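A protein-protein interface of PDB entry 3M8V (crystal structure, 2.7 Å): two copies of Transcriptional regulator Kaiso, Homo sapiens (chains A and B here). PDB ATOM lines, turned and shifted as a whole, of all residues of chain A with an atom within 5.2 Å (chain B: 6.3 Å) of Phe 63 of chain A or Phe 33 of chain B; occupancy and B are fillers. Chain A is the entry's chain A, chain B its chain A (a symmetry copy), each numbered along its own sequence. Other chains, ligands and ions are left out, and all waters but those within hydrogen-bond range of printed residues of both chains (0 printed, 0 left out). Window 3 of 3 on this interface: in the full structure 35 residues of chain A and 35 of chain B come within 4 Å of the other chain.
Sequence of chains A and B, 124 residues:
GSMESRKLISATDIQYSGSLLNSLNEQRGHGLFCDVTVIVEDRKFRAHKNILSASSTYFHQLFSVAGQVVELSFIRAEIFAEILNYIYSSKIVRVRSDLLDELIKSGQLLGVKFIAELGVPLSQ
NE2 of Gln 27 of chain B sits at hydrogen-bond distance from O of Asn 50 of chain A, 2.9 Å away.
The side-chain carboxylate of Asp 35 of chain A lies within hydrogen-bond range of the backbone NH of Lys 49 of chain A, at 2.9 Å.
The backbone carbonyl oxygen (O) of Gly 67 of chain A lies within hydrogen-bond range of the side-chain amino group (NZ) of Lys 49 of chain A (2.9 Å).
The backbone carbonyl oxygen of Gln 27 of chain B lies within hydrogen-bond range of the backbone NH of Leu 32 of chain B.
The side-chain amide oxygen of Gln 27 of chain B lies within hydrogen-bond range of a ring nitrogen (NE2) of His 48 of chain B (3.4 Å).
The backbone carbonyl oxygen (O) of Leu 32 of chain B is in hydrogen-bond range of a ring nitrogen (NE2) of His 48 of chain B (2.9 Å).
The side-chain sulfur of Cys 34 of chain B is in hydrogen-bond range of a ring nitrogen (NE2) of His 48 of chain B (3.7 Å).
Among the printed residues, merely in contact across the chains: Lys 49 of chain A with Phe 33 of chain B (3.8 Å), Asn 50 of chain A with Phe 33 of chain B (3.9 Å), Asn 50 of chain A with His 48 of chain B (3.5 Å), Ser 53 of chain A with Phe 33 of chain B (3.6 Å) and Phe 63 of chain A with Phe 33 of chain B (3.6 Å).
Phe 63 of chain A touches just one residue of chain B: Phe 33.
Phe 33 of chain B touches four residues of chain A.
Of the printed residues of chain A, His 48 of chain B touches Asn 50 (3.5 Å).
Of the printed residues of chain A, Gln 27 of chain B touches Asn 50 (2.9 Å).
Of the printed residues of chain B, Asn 50 of chain A touches Gln 27, Phe 33 and His 48.
Of the printed residues of chain B, Lys 49 of chain A touches Phe 33.
Of the printed residues of chain B, Ser 53 of chain A touches Phe 33.
Gly 67 of chain A touches none of the printed residues of chain B.
The nearest residue of chain A that does not touch Phe 33 of chain B is Asp 35 of chain A (5.1 Å).
The nearest printed residue of chain B that does not touch Lys 49 of chain A is Gln 27 of chain B (5.0 Å).
Hydrophobic or aromatic side chains of chain B that line the printed part of chain A: Phe 33 and His 48.
Hydrophobic or aromatic side chains of chain A that line the printed part of chain B: Phe 63.
Among the printed residues, 6 pairs touch across the chains.
Among the printed residues, no Asp or Glu carboxylate lies within 4 Å of a Lys or Arg side-chain nitrogen of the other chain.
3 positions are printed for both chains.
Of the 6 pairs that touch across the chains among the printed residues, none has its exchanged pair printed and touching as well.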
ATOM      1  N   ASP A  35       1.828  36.796 -15.833  1.00  0.00           N
ATOM      2  CA  ASP A  35       0.627  36.319 -16.486  1.00  0.00           C
ATOM      3  C   ASP A  35      -0.465  35.941 -15.493  1.00  0.00           C
ATOM      4  O   ASP A  35      -1.440  35.294 -15.852  1.00  0.00           O
ATOM      5  CB  ASP A  35       0.953  35.145 -17.418  1.00  0.00           C
ATOM      6  CG  ASP A  35       1.694  34.031 -16.721  1.00  0.00           C
ATOM      7  OD1 ASP A  35       2.185  34.246 -15.598  1.00  0.00           O
ATOM      8  OD2 ASP A  35       1.799  32.939 -17.312  1.00  0.00           O
ATOM      9  N   VAL A  36      -0.305  36.330 -14.237  1.00  0.00           N
ATOM     10  CA  VAL A  36      -1.390  36.124 -13.291  1.00  0.00           C
ATOM     11  C   VAL A  36      -1.400  37.221 -12.247  1.00  0.00           C
ATOM     12  O   VAL A  36      -0.375  37.825 -11.950  1.00  0.00           O
ATOM     13  CB  VAL A  36      -1.353  34.725 -12.627  1.00  0.00           C
ATOM     14  CG1 VAL A  36      -0.242  34.630 -11.630  1.00  0.00           C
ATOM     15  CG2 VAL A  36      -2.663  34.443 -11.935  1.00  0.00           C
ATOM     16  N   LYS A  49       3.028  32.462 -13.459  1.00  0.00           N
ATOM     17  CA  LYS A  49       2.496  31.112 -13.273  1.00  0.00           C
ATOM     18  C   LYS A  49       3.556  29.993 -13.262  1.00  0.00           C
ATOM     19  O   LYS A  49       3.417  29.021 -12.523  1.00  0.00           O
ATOM     20  CB  LYS A  49       1.459  30.789 -14.352  1.00  0.00           C
ATOM     21  CG  LYS A  49       0.214  31.656 -14.379  1.00  0.00           C
ATOM     22  CD  LYS A  49      -0.805  31.000 -15.312  1.00  0.00           C
ATOM     23  CE  LYS A  49      -2.066  31.810 -15.462  1.00  0.00           C
ATOM     24  NZ  LYS A  49      -2.876  31.227 -16.566  1.00  0.00           N
ATOM     25  N   ASN A  50       4.596  30.104 -14.084  1.00  0.00           N
ATOM     26  CA  ASN A  50       5.588  29.031 -14.144  1.00  0.00           C
ATOM     27  C   ASN A  50       6.334  28.898 -12.829  1.00  0.00           C
ATOM     28  O   ASN A  50       6.652  27.789 -12.397  1.00  0.00           O
ATOM     29  CB  ASN A  50       6.542  29.150 -15.369  1.00  0.00           C
ATOM     30  CG  ASN A  50       7.395  30.425 -15.372  1.00  0.00           C
ATOM     31  OD1 ASN A  50       7.159  31.375 -14.621  1.00  0.00           O
ATOM     32  ND2 ASN A  50       8.390  30.444 -16.248  1.00  0.00           N
ATOM     33  N   LEU A  52       5.106  30.049  -9.729  1.00  0.00           N
ATOM     34  CA  LEU A  52       4.196  29.673  -8.651  1.00  0.00           C
ATOM     35  C   LEU A  52       3.758  28.223  -8.766  1.00  0.00           C
ATOM     36  O   LEU A  52       3.650  27.508  -7.758  1.00  0.00           O
ATOM     37  CB  LEU A  52       2.975  30.580  -8.624  1.00  0.00           C
ATOM     38  CG  LEU A  52       3.189  32.093  -8.569  1.00  0.00           C
ATOM     39  CD1 LEU A  52       1.859  32.767  -8.313  1.00  0.00           C
ATOM     40  CD2 LEU A  52       4.178  32.448  -7.505  1.00  0.00           C
ATOM     41  N   SER A  53       3.504  27.782  -9.994  1.00  0.00           N
ATOM     42  CA  SER A  53       3.207  26.370 -10.220  1.00  0.00           C
ATOM     43  C   SER A  53       4.341  25.471  -9.709  1.00  0.00           C
ATOM     44  O   SER A  53       4.106  24.489  -9.003  1.00  0.00           O
ATOM     45  CB  SER A  53       2.907  26.096 -11.694  1.00  0.00           C
ATOM     46  OG  SER A  53       2.694  24.714 -11.920  1.00  0.00           O
ATOM     47  N   PHE A  59      -1.092  26.491  -6.271  1.00  0.00           N
ATOM     48  CA  PHE A  59      -0.990  27.134  -7.582  1.00  0.00           C
ATOM     49  C   PHE A  59      -0.735  26.147  -8.720  1.00  0.00           C
ATOM     50  O   PHE A  59      -1.153  26.384  -9.854  1.00  0.00           O
ATOM     51  CB  PHE A  59       0.107  28.195  -7.575  1.00  0.00           C
ATOM     52  CG  PHE A  59      -0.236  29.400  -6.757  1.00  0.00           C
ATOM     53  CD1 PHE A  59      -1.459  30.050  -6.930  1.00  0.00           C
ATOM     54  CD2 PHE A  59       0.646  29.876  -5.798  1.00  0.00           C
ATOM     55  CE1 PHE A  59      -1.792  31.164  -6.175  1.00  0.00           C
ATOM     56  CE2 PHE A  59       0.322  30.991  -5.033  1.00  0.00           C
ATOM     57  CZ  PHE A  59      -0.895  31.640  -5.223  1.00  0.00           C
ATOM     58  N   HIS A  60      -0.038  25.052  -8.428  1.00  0.00           N
ATOM     59  CA  HIS A  60       0.164  24.023  -9.436  1.00  0.00           C
ATOM     60  C   HIS A  60      -1.193  23.517  -9.929  1.00  0.00           C
ATOM     61  O   HIS A  60      -1.437  23.372 -11.130  1.00  0.00           O
ATOM     62  CB  HIS A  60       0.975  22.861  -8.866  1.00  0.00           C
ATOM     63  CG  HIS A  60       1.411  21.877  -9.904  1.00  0.00           C
ATOM     64  ND1 HIS A  60       0.585  20.879 -10.380  1.00  0.00           N
ATOM     65  CD2 HIS A  60       2.572  21.760 -10.590  1.00  0.00           C
ATOM     66  CE1 HIS A  60       1.226  20.182 -11.297  1.00  0.00           C
ATOM     67  NE2 HIS A  60       2.432  20.695 -11.447  1.00  0.00           N
ATOM     68  N   GLN A  61      -2.068  23.265  -8.964  1.00  0.00           N
ATOM     69  CA  GLN A  61      -3.438  22.824  -9.177  1.00  0.00           C
ATOM     70  C   GLN A  61      -4.249  23.830  -9.998  1.00  0.00           C
ATOM     71  O   GLN A  61      -4.874  23.483 -11.000  1.00  0.00           O
ATOM     72  CB  GLN A  61      -4.102  22.645  -7.810  1.00  0.00           C
ATOM     73  CG  GLN A  61      -5.534  22.207  -7.883  1.00  0.00           C
ATOM     74  CD  GLN A  61      -5.659  20.889  -8.603  1.00  0.00           C
ATOM     75  OE1 GLN A  61      -5.719  20.837  -9.835  1.00  0.00           O
ATOM     76  NE2 GLN A  61      -5.684  19.802  -7.837  1.00  0.00           N
ATOM     77  N   LEU A  62      -4.247  25.075  -9.539  1.00  0.00           N
ATOM     78  CA  LEU A  62      -4.995  26.156 -10.160  1.00  0.00           C
ATOM     79  C   LEU A  62      -4.636  26.374 -11.627  1.00  0.00           C
ATOM     80  O   LEU A  62      -5.515  26.549 -12.480  1.00  0.00           O
ATOM     81  CB  LEU A  62      -4.682  27.447  -9.406  1.00  0.00           C
ATOM     82  CG  LEU A  62      -5.826  28.242  -8.796  1.00  0.00           C
ATOM     83  CD1 LEU A  62      -6.906  27.318  -8.239  1.00  0.00           C
ATOM     84  CD2 LEU A  62      -5.269  29.157  -7.729  1.00  0.00           C
ATOM     85  N   PHE A  63      -3.332  26.380 -11.902  1.00  0.00           N
ATOM     86  CA  PHE A  63      -2.795  26.871 -13.166  1.00  0.00           C
ATOM     87  C   PHE A  63      -2.744  25.818 -14.258  1.00  0.00           C
ATOM     88  O   PHE A  63      -2.205  26.059 -15.339  1.00  0.00           O
ATOM     89  CB  PHE A  63      -1.408  27.469 -12.949  1.00  0.00           C
ATOM     90  CG  PHE A  63      -1.420  28.717 -12.124  1.00  0.00           C
ATOM     91  CD1 PHE A  63      -2.598  29.431 -11.945  1.00  0.00           C
ATOM     92  CD2 PHE A  63      -0.265  29.180 -11.522  1.00  0.00           C
ATOM     93  CE1 PHE A  63      -2.621  30.588 -11.179  1.00  0.00           C
ATOM     94  CE2 PHE A  63      -0.277  30.334 -10.758  1.00  0.00           C
ATOM     95  CZ  PHE A  63      -1.460  31.042 -10.590  1.00  0.00           C
ATOM     96  N   SER A  64      -3.291  24.648 -13.964  1.00  0.00           N
ATOM     97  CA  SER A  64      -3.487  23.618 -14.970  1.00  0.00           C
ATOM     98  C   SER A  64      -4.779  23.891 -15.748  1.00  0.00           C
ATOM     99  O   SER A  64      -5.207  23.089 -16.584  1.00  0.00           O
ATOM    100  CB  SER A  64      -3.539  22.238 -14.313  1.00  0.00           C
ATOM    101  OG  SER A  64      -4.601  22.160 -13.376  1.00  0.00           O
ATOM    102  N   VAL A  65      -5.401  25.030 -15.464  1.00  0.00           N
ATOM    103  CA  VAL A  65      -6.590  25.452 -16.192  1.00  0.00           C
ATOM    104  C   VAL A  65      -6.553  26.954 -16.408  1.00  0.00           C
ATOM    105  O   VAL A  65      -5.786  27.666 -15.765  1.00  0.00           O
ATOM    106  CB  VAL A  65      -7.897  25.099 -15.440  1.00  0.00           C
ATOM    107  CG1 VAL A  65      -7.990  23.604 -15.180  1.00  0.00           C
ATOM    108  CG2 VAL A  65      -7.992  25.882 -14.135  1.00  0.00           C
ATOM    109  N   GLY A  67      -7.245  30.884 -16.316  1.00  0.00           N
ATOM    110  CA  GLY A  67      -7.375  31.747 -15.162  1.00  0.00           C
ATOM    111  C   GLY A  67      -6.264  32.769 -15.119  1.00  0.00           C
ATOM    112  O   GLY A  67      -5.093  32.417 -15.089  1.00  0.00           O
ATOM    113  N   VAL A  70      -6.620  35.047  -9.458  1.00  0.00           N
ATOM    114  CA  VAL A  70      -7.024  34.176  -8.363  1.00  0.00           C
ATOM    115  C   VAL A  70      -7.241  34.953  -7.070  1.00  0.00           C
ATOM    116  O   VAL A  70      -6.448  35.819  -6.696  1.00  0.00           O
ATOM    117  CB  VAL A  70      -6.069  32.963  -8.163  1.00  0.00           C
ATOM    118  CG1 VAL A  70      -4.984  32.974  -9.193  1.00  0.00           C
ATOM    119  CG2 VAL A  70      -5.514  32.918  -6.743  1.00  0.00           C
ATOM    120  N   GLN B  27       8.853  21.619 -17.186  1.00  0.00           N
ATOM    121  CA  GLN B  27       7.796  22.393 -17.822  1.00  0.00           C
ATOM    122  C   GLN B  27       8.078  22.578 -19.309  1.00  0.00           C
ATOM    123  O   GLN B  27       7.201  22.388 -20.152  1.00  0.00           O
ATOM    124  CB  GLN B  27       7.645  23.768 -17.171  1.00  0.00           C
ATOM    125  CG  GLN B  27       6.937  23.796 -15.828  1.00  0.00           C
ATOM    126  CD  GLN B  27       6.976  25.183 -15.219  1.00  0.00           C
ATOM    127  OE1 GLN B  27       7.469  26.120 -15.845  1.00  0.00           O
ATOM    128  NE2 GLN B  27       6.471  25.321 -13.996  1.00  0.00           N
ATOM    129  N   GLY B  31       6.262  21.841 -22.759  1.00  0.00           N
ATOM    130  CA  GLY B  31       5.716  23.088 -23.273  1.00  0.00           C
ATOM    131  C   GLY B  31       4.848  23.838 -22.278  1.00  0.00           C
ATOM    132  O   GLY B  31       4.223  24.844 -22.617  1.00  0.00           O
ATOM    133  N   LEU B  32       4.816  23.346 -21.041  1.00  0.00           N
ATOM    134  CA  LEU B  32       4.017  23.955 -19.992  1.00  0.00           C
ATOM    135  C   LEU B  32       4.431  25.393 -19.741  1.00  0.00           C
ATOM    136  O   LEU B  32       5.587  25.671 -19.426  1.00  0.00           O
ATOM    137  CB  LEU B  32       4.128  23.148 -18.701  1.00  0.00           C
ATOM    138  CG  LEU B  32       3.044  22.104 -18.409  1.00  0.00           C
ATOM    139  CD1 LEU B  32       2.032  21.983 -19.551  1.00  0.00           C
ATOM    140  CD2 LEU B  32       3.678  20.746 -18.087  1.00  0.00           C
ATOM    141  N   PHE B  33       3.466  26.295 -19.886  1.00  0.00           N
ATOM    142  CA  PHE B  33       3.638  27.726 -19.620  1.00  0.00           C
ATOM    143  C   PHE B  33       4.580  28.416 -20.606  1.00  0.00           C
ATOM    144  O   PHE B  33       4.864  29.612 -20.480  1.00  0.00           O
ATOM    145  CB  PHE B  33       4.089  27.972 -18.171  1.00  0.00           C
ATOM    146  CG  PHE B  33       3.163  27.394 -17.134  1.00  0.00           C
ATOM    147  CD1 PHE B  33       1.880  27.889 -16.976  1.00  0.00           C
ATOM    148  CD2 PHE B  33       3.581  26.362 -16.306  1.00  0.00           C
ATOM    149  CE1 PHE B  33       1.029  27.360 -16.022  1.00  0.00           C
ATOM    150  CE2 PHE B  33       2.734  25.832 -15.349  1.00  0.00           C
ATOM    151  CZ  PHE B  33       1.456  26.329 -15.206  1.00  0.00           C
ATOM    152  N   CYS B  34       5.062  27.664 -21.591  1.00  0.00           N
ATOM    153  CA  CYS B  34       5.995  28.211 -22.574  1.00  0.00           C
ATOM    154  C   CYS B  34       5.311  29.205 -23.504  1.00  0.00           C
ATOM    155  O   CYS B  34       4.278  28.908 -24.108  1.00  0.00           O
ATOM    156  CB  CYS B  34       6.651  27.096 -23.384  1.00  0.00           C
ATOM    157  SG  CYS B  34       7.758  26.069 -22.402  1.00  0.00           S
ATOM    158  N   ASP B  35       5.899  30.386 -23.619  1.00  0.00           N
ATOM    159  CA  ASP B  35       5.285  31.446 -24.392  1.00  0.00           C
ATOM    160  C   ASP B  35       6.157  31.894 -25.558  1.00  0.00           C
ATOM    161  O   ASP B  35       5.914  32.932 -26.159  1.00  0.00           O
ATOM    162  CB  ASP B  35       4.924  32.631 -23.489  1.00  0.00           C
ATOM    163  CG  ASP B  35       6.095  33.131 -22.681  1.00  0.00           C
ATOM    164  OD1 ASP B  35       7.121  32.429 -22.610  1.00  0.00           O
ATOM    165  OD2 ASP B  35       5.979  34.226 -22.098  1.00  0.00           O
ATOM    166  N   VAL B  36       7.186  31.124 -25.880  1.00  0.00           N
ATOM    167  CA  VAL B  36       7.953  31.431 -27.076  1.00  0.00           C
ATOM    168  C   VAL B  36       8.496  30.163 -27.700  1.00  0.00           C
ATOM    169  O   VAL B  36       8.707  29.162 -27.024  1.00  0.00           O
ATOM    170  CB  VAL B  36       9.086  32.455 -26.818  1.00  0.00           C
ATOM    171  CG1 VAL B  36      10.212  31.831 -26.055  1.00  0.00           C
ATOM    172  CG2 VAL B  36       9.613  32.988 -28.127  1.00  0.00           C
ATOM    173  N   ALA B  47      10.001  27.422 -24.940  1.00  0.00           N
ATOM    174  CA  ALA B  47      10.605  27.970 -23.726  1.00  0.00           C
ATOM    175  C   ALA B  47       9.811  29.107 -23.074  1.00  0.00           C
ATOM    176  O   ALA B  47       8.738  29.482 -23.547  1.00  0.00           O
ATOM    177  CB  ALA B  47      12.032  28.420 -24.007  1.00  0.00           C
ATOM    178  N   HIS B  48      10.355  29.633 -21.975  1.00  0.00           N
ATOM    179  CA  HIS B  48       9.752  30.740 -21.231  1.00  0.00           C
ATOM    180  C   HIS B  48      10.533  32.040 -21.373  1.00  0.00           C
ATOM    181  O   HIS B  48      11.691  32.131 -20.953  1.00  0.00           O
ATOM    182  CB  HIS B  48       9.688  30.426 -19.738  1.00  0.00           C
ATOM    183  CG  HIS B  48       9.141  29.080 -19.417  1.00  0.00           C
ATOM    184  ND1 HIS B  48       9.945  27.989 -19.178  1.00  0.00           N
ATOM    185  CD2 HIS B  48       7.862  28.649 -19.265  1.00  0.00           C
ATOM    186  CE1 HIS B  48       9.190  26.943 -18.900  1.00  0.00           C
ATOM    187  NE2 HIS B  48       7.931  27.311 -18.946  1.00  0.00           N
ATOM    188  N   LYS B  49       9.875  33.058 -21.918  1.00  0.00           N
ATOM    189  CA  LYS B  49      10.463  34.391 -22.060  1.00  0.00           C
ATOM    190  C   LYS B  49      11.061  34.978 -20.767  1.00  0.00           C
ATOM    191  O   LYS B  49      12.076  35.669 -20.816  1.00  0.00           O
ATOM    192  CB  LYS B  49       9.430  35.378 -22.610  1.00  0.00           C
ATOM    193  CG  LYS B  49       8.882  35.087 -23.994  1.00  0.00           C
ATOM    194  CD  LYS B  49       8.109  36.318 -24.471  1.00  0.00           C
ATOM    195  CE  LYS B  49       7.467  36.118 -25.818  1.00  0.00           C
ATOM    196  NZ  LYS B  49       6.545  37.257 -26.078  1.00  0.00           N
